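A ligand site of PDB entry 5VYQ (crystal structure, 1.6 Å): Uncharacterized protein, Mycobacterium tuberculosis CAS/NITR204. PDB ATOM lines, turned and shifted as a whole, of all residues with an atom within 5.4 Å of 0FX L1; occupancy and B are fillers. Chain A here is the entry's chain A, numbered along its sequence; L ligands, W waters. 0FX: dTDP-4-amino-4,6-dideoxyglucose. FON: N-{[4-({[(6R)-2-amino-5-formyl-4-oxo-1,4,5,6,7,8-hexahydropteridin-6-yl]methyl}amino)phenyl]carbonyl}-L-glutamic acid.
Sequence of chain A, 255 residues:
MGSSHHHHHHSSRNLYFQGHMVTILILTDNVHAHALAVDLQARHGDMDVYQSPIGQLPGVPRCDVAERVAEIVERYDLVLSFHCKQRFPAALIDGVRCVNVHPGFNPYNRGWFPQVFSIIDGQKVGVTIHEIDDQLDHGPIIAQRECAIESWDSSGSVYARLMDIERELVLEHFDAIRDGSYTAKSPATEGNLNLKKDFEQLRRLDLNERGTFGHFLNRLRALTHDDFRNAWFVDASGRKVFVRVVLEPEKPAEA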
ATOM      1  N   ASN A  30     -21.382   1.066  -0.978  1.00  0.00           N
ATOM      2  CA  ASN A  30     -20.438   0.116  -0.362  1.00  0.00           C
ATOM      3  C   ASN A  30     -19.699  -0.653  -1.463  1.00  0.00           C
ATOM      4  O   ASN A  30     -20.290  -1.120  -2.433  1.00  0.00           O
ATOM      5  CB  ASN A  30     -21.211  -0.849   0.556  1.00  0.00           C
ATOM      6  CG  ASN A  30     -20.350  -1.939   1.147  1.00  0.00           C
ATOM      7  OD1 ASN A  30     -20.050  -2.921   0.482  1.00  0.00           O
ATOM      8  ND2 ASN A  30     -19.986  -1.807   2.416  1.00  0.00           N
ATOM      9  N   HIS A  83     -26.897  -1.356   0.346  1.00  0.00           N
ATOM     10  CA  HIS A  83     -26.203  -0.529   1.294  1.00  0.00           C
ATOM     11  C   HIS A  83     -26.149   0.924   0.816  1.00  0.00           C
ATOM     12  O   HIS A  83     -25.087   1.570   0.840  1.00  0.00           O
ATOM     13  CB  HIS A  83     -24.757  -0.956   1.572  1.00  0.00           C
ATOM     14  CG  HIS A  83     -24.540  -2.377   2.037  1.00  0.00           C
ATOM     15  ND1 HIS A  83     -23.429  -2.698   2.785  1.00  0.00           N
ATOM     16  CD2 HIS A  83     -25.188  -3.546   1.795  1.00  0.00           C
ATOM     17  CE1 HIS A  83     -23.416  -4.008   2.999  1.00  0.00           C
ATOM     18  NE2 HIS A  83     -24.485  -4.538   2.435  1.00  0.00           N
ATOM     19  N   CYS A  84     -27.279   1.455   0.357  1.00  0.00           N
ATOM     20  CA  CYS A  84     -27.404   2.868   0.097  1.00  0.00           C
ATOM     21  C   CYS A  84     -27.521   3.615   1.415  1.00  0.00           C
ATOM     22  O   CYS A  84     -28.362   3.266   2.247  1.00  0.00           O
ATOM     23  CB  CYS A  84     -28.676   3.107  -0.729  1.00  0.00           C
ATOM     24  SG  CYS A  84     -28.957   4.842  -1.108  1.00  0.00           S
ATOM     25  N   LYS A  85     -26.710   4.641   1.601  1.00  0.00           N
ATOM     26  CA  LYS A  85     -26.702   5.369   2.868  1.00  0.00           C
ATOM     27  C   LYS A  85     -27.769   6.457   2.930  1.00  0.00           C
ATOM     28  O   LYS A  85     -28.129   6.883   4.045  1.00  0.00           O
ATOM     29  CB  LYS A  85     -25.320   5.997   3.176  1.00  0.00           C
ATOM     30  CG  LYS A  85     -24.232   4.977   3.473  1.00  0.00           C
ATOM     31  CD  LYS A  85     -24.037   4.712   4.968  1.00  0.00           C
ATOM     32  CE  LYS A  85     -22.872   3.793   5.358  1.00  0.00           C
ATOM     33  NZ  LYS A  85     -21.585   4.021   4.636  1.00  0.00           N
ATOM     34  N   ASN A 100     -34.321  -3.772   0.216  1.00  0.00           N
ATOM     35  CA  ASN A 100     -33.055  -3.565   0.864  1.00  0.00           C
ATOM     36  C   ASN A 100     -32.333  -4.874   1.090  1.00  0.00           C
ATOM     37  O   ASN A 100     -32.935  -5.884   1.435  1.00  0.00           O
ATOM     38  CB  ASN A 100     -33.322  -2.916   2.224  1.00  0.00           C
ATOM     39  CG  ASN A 100     -32.074  -2.407   2.886  1.00  0.00           C
ATOM     40  OD1 ASN A 100     -31.184  -1.832   2.248  1.00  0.00           O
ATOM     41  ND2 ASN A 100     -32.020  -2.508   4.222  1.00  0.00           N
ATOM     42  N   VAL A 101     -31.014  -4.827   0.876  1.00  0.00           N
ATOM     43  CA  VAL A 101     -30.143  -5.880   1.301  1.00  0.00           C
ATOM     44  C   VAL A 101     -29.290  -5.387   2.466  1.00  0.00           C
ATOM     45  O   VAL A 101     -28.445  -4.512   2.300  1.00  0.00           O
ATOM     46  CB  VAL A 101     -29.226  -6.344   0.162  1.00  0.00           C
ATOM     47  CG1 VAL A 101     -28.259  -7.399   0.682  1.00  0.00           C
ATOM     48  CG2 VAL A 101     -30.051  -6.781  -1.049  1.00  0.00           C
ATOM     49  N   HIS A 102     -29.616  -5.915   3.618  1.00  0.00           N
ATOM     50  CA  HIS A 102     -29.147  -5.391   4.905  1.00  0.00           C
ATOM     51  C   HIS A 102     -28.237  -6.395   5.596  1.00  0.00           C
ATOM     52  O   HIS A 102     -28.637  -7.573   5.814  1.00  0.00           O
ATOM     53  CB  HIS A 102     -30.320  -5.159   5.821  1.00  0.00           C
ATOM     54  CG  HIS A 102     -29.980  -4.797   7.235  1.00  0.00           C
ATOM     55  ND1 HIS A 102     -29.203  -3.700   7.580  1.00  0.00           N
ATOM     56  CD2 HIS A 102     -30.378  -5.356   8.400  1.00  0.00           C
ATOM     57  CE1 HIS A 102     -29.103  -3.646   8.890  1.00  0.00           C
ATOM     58  NE2 HIS A 102     -29.791  -4.645   9.412  1.00  0.00           N
ATOM     59  N   PRO A 103     -27.028  -5.935   5.974  1.00  0.00           N
ATOM     60  CA  PRO A 103     -26.094  -6.829   6.649  1.00  0.00           C
ATOM     61  C   PRO A 103     -26.338  -6.928   8.174  1.00  0.00           C
ATOM     62  O   PRO A 103     -25.429  -6.784   8.999  1.00  0.00           O
ATOM     63  CB  PRO A 103     -24.734  -6.215   6.276  1.00  0.00           C
ATOM     64  CG  PRO A 103     -25.032  -4.755   6.300  1.00  0.00           C
ATOM     65  CD  PRO A 103     -26.421  -4.628   5.700  1.00  0.00           C
ATOM     66  N   GLY A 111     -30.249  -1.144  11.835  1.00  0.00           N
ATOM     67  CA  GLY A 111     -29.553   0.130  11.731  1.00  0.00           C
ATOM     68  C   GLY A 111     -28.055  -0.119  11.666  1.00  0.00           C
ATOM     69  O   GLY A 111     -27.526  -0.943  10.905  1.00  0.00           O
ATOM     70  N   TRP A 112     -27.326   0.605  12.465  1.00  0.00           N
ATOM     71  CA  TRP A 112     -25.927   0.835  12.167  1.00  0.00           C
ATOM     72  C   TRP A 112     -25.036  -0.322  12.646  1.00  0.00           C
ATOM     73  O   TRP A 112     -25.149  -0.775  13.764  1.00  0.00           O
ATOM     74  CB  TRP A 112     -25.542   2.132  12.911  1.00  0.00           C
ATOM     75  CG  TRP A 112     -24.418   2.844  12.339  1.00  0.00           C
ATOM     76  CD1 TRP A 112     -23.155   2.887  12.838  1.00  0.00           C
ATOM     77  CD2 TRP A 112     -24.411   3.614  11.123  1.00  0.00           C
ATOM     78  NE1 TRP A 112     -22.363   3.674  12.025  1.00  0.00           N
ATOM     79  CE2 TRP A 112     -23.104   4.125  10.974  1.00  0.00           C
ATOM     80  CE3 TRP A 112     -25.380   3.932  10.168  1.00  0.00           C
ATOM     81  CZ2 TRP A 112     -22.725   4.913   9.873  1.00  0.00           C
ATOM     82  CZ3 TRP A 112     -25.008   4.715   9.073  1.00  0.00           C
ATOM     83  CH2 TRP A 112     -23.701   5.202   8.940  1.00  0.00           C
ATOM     84  N   PHE A 113     -24.174  -0.803  11.768  1.00  0.00           N
ATOM     85  CA  PHE A 113     -23.120  -1.761  12.068  1.00  0.00           C
ATOM     86  C   PHE A 113     -23.605  -2.947  12.925  1.00  0.00           C
ATOM     87  O   PHE A 113     -23.132  -3.191  14.019  1.00  0.00           O
ATOM     88  CB  PHE A 113     -21.923  -1.102  12.718  1.00  0.00           C
ATOM     89  CG  PHE A 113     -21.303   0.032  11.936  1.00  0.00           C
ATOM     90  CD1 PHE A 113     -21.626   0.326  10.614  1.00  0.00           C
ATOM     91  CD2 PHE A 113     -20.289   0.780  12.548  1.00  0.00           C
ATOM     92  CE1 PHE A 113     -21.019   1.376   9.946  1.00  0.00           C
ATOM     93  CE2 PHE A 113     -19.619   1.792  11.877  1.00  0.00           C
ATOM     94  CZ  PHE A 113     -19.998   2.095  10.562  1.00  0.00           C
ATOM     95  N   PRO A 114     -24.567  -3.694  12.392  1.00  0.00           N
ATOM     96  CA  PRO A 114     -25.180  -4.701  13.287  1.00  0.00           C
ATOM     97  C   PRO A 114     -24.237  -5.651  14.053  1.00  0.00           C
ATOM     98  O   PRO A 114     -24.529  -5.977  15.215  1.00  0.00           O
ATOM     99  CB  PRO A 114     -26.086  -5.489  12.335  1.00  0.00           C
ATOM    100  CG  PRO A 114     -26.543  -4.439  11.349  1.00  0.00           C
ATOM    101  CD  PRO A 114     -25.298  -3.589  11.118  1.00  0.00           C
ATOM    102  N   GLN A 115     -23.214  -6.175  13.388  1.00  0.00           N
ATOM    103  CA  GLN A 115     -22.342  -7.197  14.022  1.00  0.00           C
ATOM    104  C   GLN A 115     -21.597  -6.586  15.222  1.00  0.00           C
ATOM    105  O   GLN A 115     -21.258  -7.319  16.146  1.00  0.00           O
ATOM    106  CB  GLN A 115     -21.318  -7.804  13.049  1.00  0.00           C
ATOM    107  CG  GLN A 115     -20.122  -6.938  12.601  1.00  0.00           C
ATOM    108  CD  GLN A 115     -20.473  -5.871  11.600  1.00  0.00           C
ATOM    109  OE1 GLN A 115     -21.589  -5.872  11.034  1.00  0.00           O
ATOM    110  NE2 GLN A 115     -19.577  -4.920  11.429  1.00  0.00           N
ATOM    111  N   VAL A 116     -21.321  -5.284  15.213  1.00  0.00           N
ATOM    112  CA  VAL A 116     -20.682  -4.631  16.348  1.00  0.00           C
ATOM    113  C   VAL A 116     -21.548  -4.841  17.583  1.00  0.00           C
ATOM    114  O   VAL A 116     -21.106  -5.315  18.620  1.00  0.00           O
ATOM    115  CB  VAL A 116     -20.414  -3.130  16.125  1.00  0.00           C
ATOM    116  CG1 VAL A 116     -19.907  -2.505  17.391  1.00  0.00           C
ATOM    117  CG2 VAL A 116     -19.483  -2.911  14.940  1.00  0.00           C
ATOM    118  N   ASP A 137     -34.675  -0.690   8.265  1.00  0.00           N
ATOM    119  CA  ASP A 137     -34.428  -2.094   8.353  1.00  0.00           C
ATOM    120  C   ASP A 137     -35.632  -2.764   8.992  1.00  0.00           C
ATOM    121  O   ASP A 137     -35.518  -3.491   9.975  1.00  0.00           O
ATOM    122  CB  ASP A 137     -33.145  -2.372   9.115  1.00  0.00           C
ATOM    123  CG  ASP A 137     -31.940  -1.702   8.476  1.00  0.00           C
ATOM    124  OD1 ASP A 137     -31.870  -1.588   7.246  1.00  0.00           O
ATOM    125  OD2 ASP A 137     -31.034  -1.338   9.225  1.00  0.00           O
ATOM    126  N   SER A 155     -15.463  -7.520  14.750  1.00  0.00           N
ATOM    127  CA  SER A 155     -16.326  -6.909  13.730  1.00  0.00           C
ATOM    128  C   SER A 155     -15.814  -7.185  12.303  1.00  0.00           C
ATOM    129  O   SER A 155     -16.558  -7.582  11.385  1.00  0.00           O
ATOM    130  CB  SER A 155     -16.502  -5.426  13.982  1.00  0.00           C
ATOM    131  OG  SER A 155     -17.114  -4.822  12.850  1.00  0.00           O
ATOM    132  N   TYR A 159     -17.817  -9.351   9.483  1.00  0.00           N
ATOM    133  CA  TYR A 159     -18.281  -8.564   8.346  1.00  0.00           C
ATOM    134  C   TYR A 159     -17.835  -9.199   7.021  1.00  0.00           C
ATOM    135  O   TYR A 159     -18.611  -9.259   6.073  1.00  0.00           O
ATOM    136  CB  TYR A 159     -17.715  -7.143   8.440  1.00  0.00           C
ATOM    137  CG  TYR A 159     -18.339  -6.198   7.456  1.00  0.00           C
ATOM    138  CD1 TYR A 159     -19.636  -5.749   7.589  1.00  0.00           C
ATOM    139  CD2 TYR A 159     -17.640  -5.817   6.340  1.00  0.00           C
ATOM    140  CE1 TYR A 159     -20.190  -4.882   6.653  1.00  0.00           C
ATOM    141  CE2 TYR A 159     -18.175  -4.987   5.385  1.00  0.00           C
ATOM    142  CZ  TYR A 159     -19.457  -4.523   5.547  1.00  0.00           C
ATOM    143  OH  TYR A 159     -20.004  -3.677   4.639  1.00  0.00           O
ATOM    144  N   MET A 163     -20.384 -10.341   4.008  1.00  0.00           N
ATOM    145  CA  MET A 163     -20.368  -9.967   2.585  1.00  0.00           C
ATOM    146  C   MET A 163     -20.445 -11.246   1.727  1.00  0.00           C
ATOM    147  O   MET A 163     -21.059 -11.207   0.650  1.00  0.00           O
ATOM    148  CB  MET A 163     -19.127  -9.163   2.266  1.00  0.00           C
ATOM    149  CG  MET A 163     -19.018  -7.811   2.974  1.00  0.00           C
ATOM    150  SD  MET A 163     -20.372  -6.700   2.659  1.00  0.00           S
ATOM    151  CE  MET A 163     -21.552  -7.198   3.885  1.00  0.00           C
ATOM    152  N   PHE A 199     -23.217   3.875  18.014  1.00  0.00           N
ATOM    153  CA  PHE A 199     -21.869   3.387  17.745  1.00  0.00           C
ATOM    154  C   PHE A 199     -20.829   4.394  18.224  1.00  0.00           C
ATOM    155  O   PHE A 199     -19.856   4.042  18.907  1.00  0.00           O
ATOM    156  CB  PHE A 199     -21.685   3.141  16.236  1.00  0.00           C
ATOM    157  CG  PHE A 199     -20.316   2.699  15.887  1.00  0.00           C
ATOM    158  CD1 PHE A 199     -19.910   1.411  16.176  1.00  0.00           C
ATOM    159  CD2 PHE A 199     -19.422   3.570  15.304  1.00  0.00           C
ATOM    160  CE1 PHE A 199     -18.631   0.992  15.870  1.00  0.00           C
ATOM    161  CE2 PHE A 199     -18.164   3.139  14.999  1.00  0.00           C
ATOM    162  CZ  PHE A 199     -17.757   1.876  15.288  1.00  0.00           C
ATOM    163  N   HIS A 225     -11.926  -3.767  13.720  1.00  0.00           N
ATOM    164  CA  HIS A 225     -12.352  -3.926  12.325  1.00  0.00           C
ATOM    165  C   HIS A 225     -11.249  -3.474  11.401  1.00  0.00           C
ATOM    166  O   HIS A 225     -11.119  -2.279  11.145  1.00  0.00           O
ATOM    167  CB  HIS A 225     -13.637  -3.133  12.045  1.00  0.00           C
ATOM    168  CG  HIS A 225     -14.308  -3.532  10.773  1.00  0.00           C
ATOM    169  ND1 HIS A 225     -15.553  -4.130  10.733  1.00  0.00           N
ATOM    170  CD2 HIS A 225     -13.873  -3.469   9.484  1.00  0.00           C
ATOM    171  CE1 HIS A 225     -15.877  -4.345   9.472  1.00  0.00           C
ATOM    172  NE2 HIS A 225     -14.891  -3.946   8.695  1.00  0.00           N
ATOM    173  N   PHE A 228      -9.388   0.241  11.335  1.00  0.00           N
ATOM    174  CA  PHE A 228     -10.178   1.345  11.840  1.00  0.00           C
ATOM    175  C   PHE A 228      -9.809   1.673  13.281  1.00  0.00           C
ATOM    176  O   PHE A 228      -9.697   0.806  14.134  1.00  0.00           O
ATOM    177  CB  PHE A 228     -11.688   1.094  11.806  1.00  0.00           C
ATOM    178  CG  PHE A 228     -12.321   1.281  10.432  1.00  0.00           C
ATOM    179  CD1 PHE A 228     -12.447   2.538   9.862  1.00  0.00           C
ATOM    180  CD2 PHE A 228     -12.825   0.192   9.738  1.00  0.00           C
ATOM    181  CE1 PHE A 228     -13.068   2.716   8.633  1.00  0.00           C
ATOM    182  CE2 PHE A 228     -13.433   0.337   8.501  1.00  0.00           C
ATOM    183  CZ  PHE A 228     -13.565   1.614   7.955  1.00  0.00           C
ATOM    184  N   ASN A 230     -11.402   2.696  15.964  1.00  0.00           N
ATOM    185  CA  ASN A 230     -12.701   2.868  16.553  1.00  0.00           C
ATOM    186  C   ASN A 230     -12.673   3.099  18.066  1.00  0.00           C
ATOM    187  O   ASN A 230     -13.213   4.074  18.542  1.00  0.00           O
ATOM    188  CB  ASN A 230     -13.592   1.626  16.294  1.00  0.00           C
ATOM    189  CG  ASN A 230     -13.965   1.409  14.838  1.00  0.00           C
ATOM    190  OD1 ASN A 230     -14.284   2.346  14.076  1.00  0.00           O
ATOM    191  ND2 ASN A 230     -13.969   0.165  14.448  1.00  0.00           N
HETATM  192  O4P 0FX L   1     -21.919  -2.208   5.662  1.00  0.00           O
HETATM  193  P2  0FX L   1     -22.348  -0.798   5.412  1.00  0.00           P
HETATM  194  O3P 0FX L   1     -22.423  -0.367   3.970  1.00  0.00           O
HETATM  195  O1G 0FX L   1     -23.719  -0.716   6.261  1.00  0.00           O
HETATM  196  C1G 0FX L   1     -24.221   0.501   6.794  1.00  0.00           C
HETATM  197  C2G 0FX L   1     -25.174   0.128   7.935  1.00  0.00           C
HETATM  198  O2G 0FX L   1     -24.398  -0.661   8.849  1.00  0.00           O
HETATM  199  C3G 0FX L   1     -26.317  -0.748   7.388  1.00  0.00           C
HETATM  200  O3G 0FX L   1     -27.135  -1.278   8.463  1.00  0.00           O
HETATM  201  C4G 0FX L   1     -27.062   0.040   6.322  1.00  0.00           C
HETATM  202  N4A 0FX L   1     -28.107  -0.864   5.788  1.00  0.00           N
HETATM  203  C5G 0FX L   1     -26.070   0.487   5.245  1.00  0.00           C
HETATM  204  C6G 0FX L   1     -26.758   1.521   4.364  1.00  0.00           C
HETATM  205  O5G 0FX L   1     -24.933   1.192   5.754  1.00  0.00           O
HETATM  206  OPP 0FX L   1     -21.445   0.250   6.232  1.00  0.00           O
HETATM  207  P   0FX L   1     -19.923   0.737   5.965  1.00  0.00           P
HETATM  208  O1P 0FX L   1     -19.893   2.173   6.314  1.00  0.00           O
HETATM  209  O2P 0FX L   1     -19.473   0.216   4.620  1.00  0.00           O
HETATM  210  O5  0FX L   1     -19.057  -0.059   7.050  1.00  0.00           O
HETATM  211  C5  0FX L   1     -18.816  -1.449   6.937  1.00  0.00           C
HETATM  212  C4  0FX L   1     -18.266  -1.967   8.258  1.00  0.00           C
HETATM  213  O4  0FX L   1     -17.007  -1.337   8.489  1.00  0.00           O
HETATM  214  C3  0FX L   1     -19.071  -1.624   9.517  1.00  0.00           C
HETATM  215  O3  0FX L   1     -20.101  -2.592   9.738  1.00  0.00           O
HETATM  216  C2  0FX L   1     -18.058  -1.654  10.652  1.00  0.00           C
HETATM  217  C1  0FX L   1     -16.849  -1.153   9.904  1.00  0.00           C
HETATM  218  N11 0FX L   1     -16.610   0.280  10.142  1.00  0.00           N
HETATM  219  C61 0FX L   1     -16.876   1.259   9.252  1.00  0.00           C
HETATM  220  C51 0FX L   1     -16.597   2.583   9.532  1.00  0.00           C
HETATM  221  C5A 0FX L   1     -16.948   3.649   8.531  1.00  0.00           C
HETATM  222  C21 0FX L   1     -15.896   0.644  11.274  1.00  0.00           C
HETATM  223  O21 0FX L   1     -15.574  -0.304  12.134  1.00  0.00           O
HETATM  224  N31 0FX L   1     -15.611   1.906  11.587  1.00  0.00           N
HETATM  225  C41 0FX L   1     -15.906   2.878  10.691  1.00  0.00           C
HETATM  226  O41 0FX L   1     -15.585   4.142  11.014  1.00  0.00           O
HETATM  227  N1  FON L   2     -34.780   4.047   3.498  1.00  0.00           N
HETATM  228  C2  FON L   2     -35.759   3.635   4.292  1.00  0.00           C
HETATM  229  NA2 FON L   2     -36.942   4.305   4.255  1.00  0.00           N
HETATM  230  N3  FON L   2     -35.553   2.610   5.132  1.00  0.00           N
HETATM  231  C4  FON L   2     -34.376   1.935   5.210  1.00  0.00           C
HETATM  232  O4  FON L   2     -34.235   0.951   5.983  1.00  0.00           O
HETATM  233  C4A FON L   2     -33.281   2.334   4.307  1.00  0.00           C
HETATM  234  N5  FON L   2     -31.997   1.793   4.282  1.00  0.00           N
HETATM  235  C6  FON L   2     -30.942   2.713   3.804  1.00  0.00           C
HETATM  236  C7  FON L   2     -31.360   3.207   2.421  1.00  0.00           C
HETATM  237  N8  FON L   2     -32.645   3.856   2.536  1.00  0.00           N
HETATM  238  C8A FON L   2     -33.571   3.453   3.415  1.00  0.00           C
HETATM  239  C9  FON L   2     -30.660   3.872   4.791  1.00  0.00           C
HETATM  240  N10 FON L   2     -30.086   3.315   6.012  1.00  0.00           N
HETATM  241  C11 FON L   2     -28.978   5.594   9.319  1.00  0.00           C
HETATM  242  C12 FON L   2     -28.888   4.205   9.349  1.00  0.00           C
HETATM  243  C13 FON L   2     -29.267   3.465   8.226  1.00  0.00           C
HETATM  244  C14 FON L   2     -29.708   4.089   7.072  1.00  0.00           C
HETATM  245  C15 FON L   2     -29.806   5.475   7.031  1.00  0.00           C
HETATM  246  C16 FON L   2     -29.441   6.223   8.160  1.00  0.00           C
HETATM  247  C   FON L   2     -28.557   6.390  10.563  1.00  0.00           C
HETATM  248  O   FON L   2     -27.963   5.872  11.531  1.00  0.00           O
HETATM  249  N   FON L   2     -28.840   7.699  10.572  1.00  0.00           N
HETATM  250  CA  FON L   2     -28.422   8.606  11.634  1.00  0.00           C
HETATM  251  CB  FON L   2     -27.607   9.801  11.108  1.00  0.00           C
HETATM  252  CG  FON L   2     -26.359   9.279  10.390  1.00  0.00           C
HETATM  253  CD  FON L   2     -25.223  10.256  10.166  1.00  0.00           C
HETATM  254  OE1 FON L   2     -25.124  11.247  10.923  1.00  0.00           O
HETATM  255  OE2 FON L   2     -24.382  10.022   9.261  1.00  0.00           O
HETATM  256  CT  FON L   2     -29.635   9.073  12.389  1.00  0.00           C
HETATM  257  O1  FON L   2     -29.427   9.553  13.522  1.00  0.00           O
HETATM  258  O2  FON L   2     -30.768   8.949  11.855  1.00  0.00           O
HETATM  259  CP1 FON L   2     -31.754   0.614   4.671  1.00  0.00           C
HETATM  260  O3  FON L   2     -30.616   0.147   4.675  1.00  0.00           O
HETATM  261  O   HOH W   1     -30.009   0.507   7.745  1.00  0.00           O
HETATM  262  O   HOH W   2     -28.470  -1.911   3.051  1.00  0.00           O
HETATM  263  O   HOH W   3     -19.388   2.034   2.579  1.00  0.00           O
HETATM  264  O   HOH W   4     -15.802  -2.111  14.775  1.00  0.00           O
HETATM  265  O   HOH W   5     -14.455   5.094  13.887  1.00  0.00           O
HETATM  266  O   HOH W   6     -22.731   1.791   2.539  1.00  0.00           O
HETATM  267  O   HOH W   7     -22.568  -2.655   8.352  1.00  0.00           O
HETATM  268  O   HOH W   8     -17.666   3.547   4.622  1.00  0.00           O
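ND2 of Asn 30 is in hydrogen-bond range of O2P of 0FX L1 (3.0 Å). A ring nitrogen (ND1) of His 102 lies close to an oxygen (O3G) of 0FX L1, at 3.3 Å. The backbone NH of Phe 113 is in hydrogen-bond range of an oxygen (O2G) of 0FX L1 (2.9 Å). A ring nitrogen (NE2) of His 225 sits close to an oxygen (O4) of 0FX L1 (3.4 Å). An oxygen (O3G) of 0FX L1 sits at hydrogen-bond distance from the backbone carbonyl oxygen of Gly 111, 2.5 Å away. ND1 of His 83 is in hydrogen-bond range of O3P of 0FX L1 (2.8 Å). The side-chain amide nitrogen of Gln 115 lies within hydrogen-bond range of an oxygen (O3) of 0FX L1. The side-chain amino group (NZ) of Lys 85 lies within salt-bridge range of an oxygen (O1P) of 0FX L1, 3.0 Å away. The backbone NH of Asp 137 is in hydrogen-bond range of an oxygen (O4) of FON L2 (2.8 Å). ND2 of Asn 100 lies within hydrogen-bond range of O3 of FON L2 (3.0 Å). The side-chain amide nitrogen of Asn 230 is in hydrogen-bond range of an oxygen (O21) of 0FX L1, 2.9 Å away. The side-chain hydroxyl (OH) of Tyr 159 sits at hydrogen-bond distance from an oxygen (O4P) of 0FX L1 (2.6 Å).
A nitrogen (N4A) of 0FX L1 lies within hydrogen-bond range of an oxygen (O3) of FON L2 (2.9 Å).
OD2 of Asp 137 sits close to ND1 of His 102 (3.4 Å). The side-chain hydroxyl (OH) of Tyr 159 is in hydrogen-bond range of the side-chain sulfur (SD) of Met 163 (3.6 Å). N of Gly 111 is in hydrogen-bond range of OD2 of Asp 137. The side-chain hydroxyl (OG) of Ser 155 is in hydrogen-bond range of a ring nitrogen (ND1) of His 225 (2.7 Å). The side-chain amide nitrogen (ND2) of Asn 100 lies within hydrogen-bond range of the side-chain carboxylate (OD1) of Asp 137. The side-chain amide nitrogen (ND2) of Asn 30 is in hydrogen-bond range of the side-chain hydroxyl (OH) of Tyr 159 (2.9 Å). OG of Ser 155 sits at hydrogen-bond distance from NE2 of Gln 115.
Residues that only touch 0FX L1: Cys 84, Phe 228, Pro 114, Trp 112, Ser 155 and Asp 137. Hydrophobic or aromatic side chains that line 0FX L1: His 83, His 102, Phe 113, Pro 114, Tyr 159, His 225 and Phe 228. 16 residues have an atom within 4 Å of 0FX L1: Asn 30, His 83, Cys 84, Lys 85, His 102, Gly 111, Trp 112, Phe 113, Pro 114, Gln 115, Asp 137, Ser 155, Tyr 159, His 225, Phe 228 and Asn 230. The nearest printed residue that does not touch 0FX L1 is Pro 103 (4.1 Å).
Water W6 lies within hydrogen-bond range of O3P of 0FX L1 (2.6 Å), O of His 83 (2.9 Å) and NZ of Lys 85 (3.3 Å). Water W1 lies within hydrogen-bond range of the side-chain carboxylate of Asp 137 (2.6 Å), a nitrogen (N4A) of 0FX L1 (3.1 Å) and an oxygen (O3) of FON L2 (3.2 Å). Water W4 lies within hydrogen-bond range of the side-chain amide nitrogen (ND2) of Asn 230 (2.9 Å) and an oxygen (O21) of 0FX L1 (3.2 Å). Water W5 lies within hydrogen-bond range of OD1 of Asn 230 (2.8 Å) and O41 of 0FX L1 (3.2 Å).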
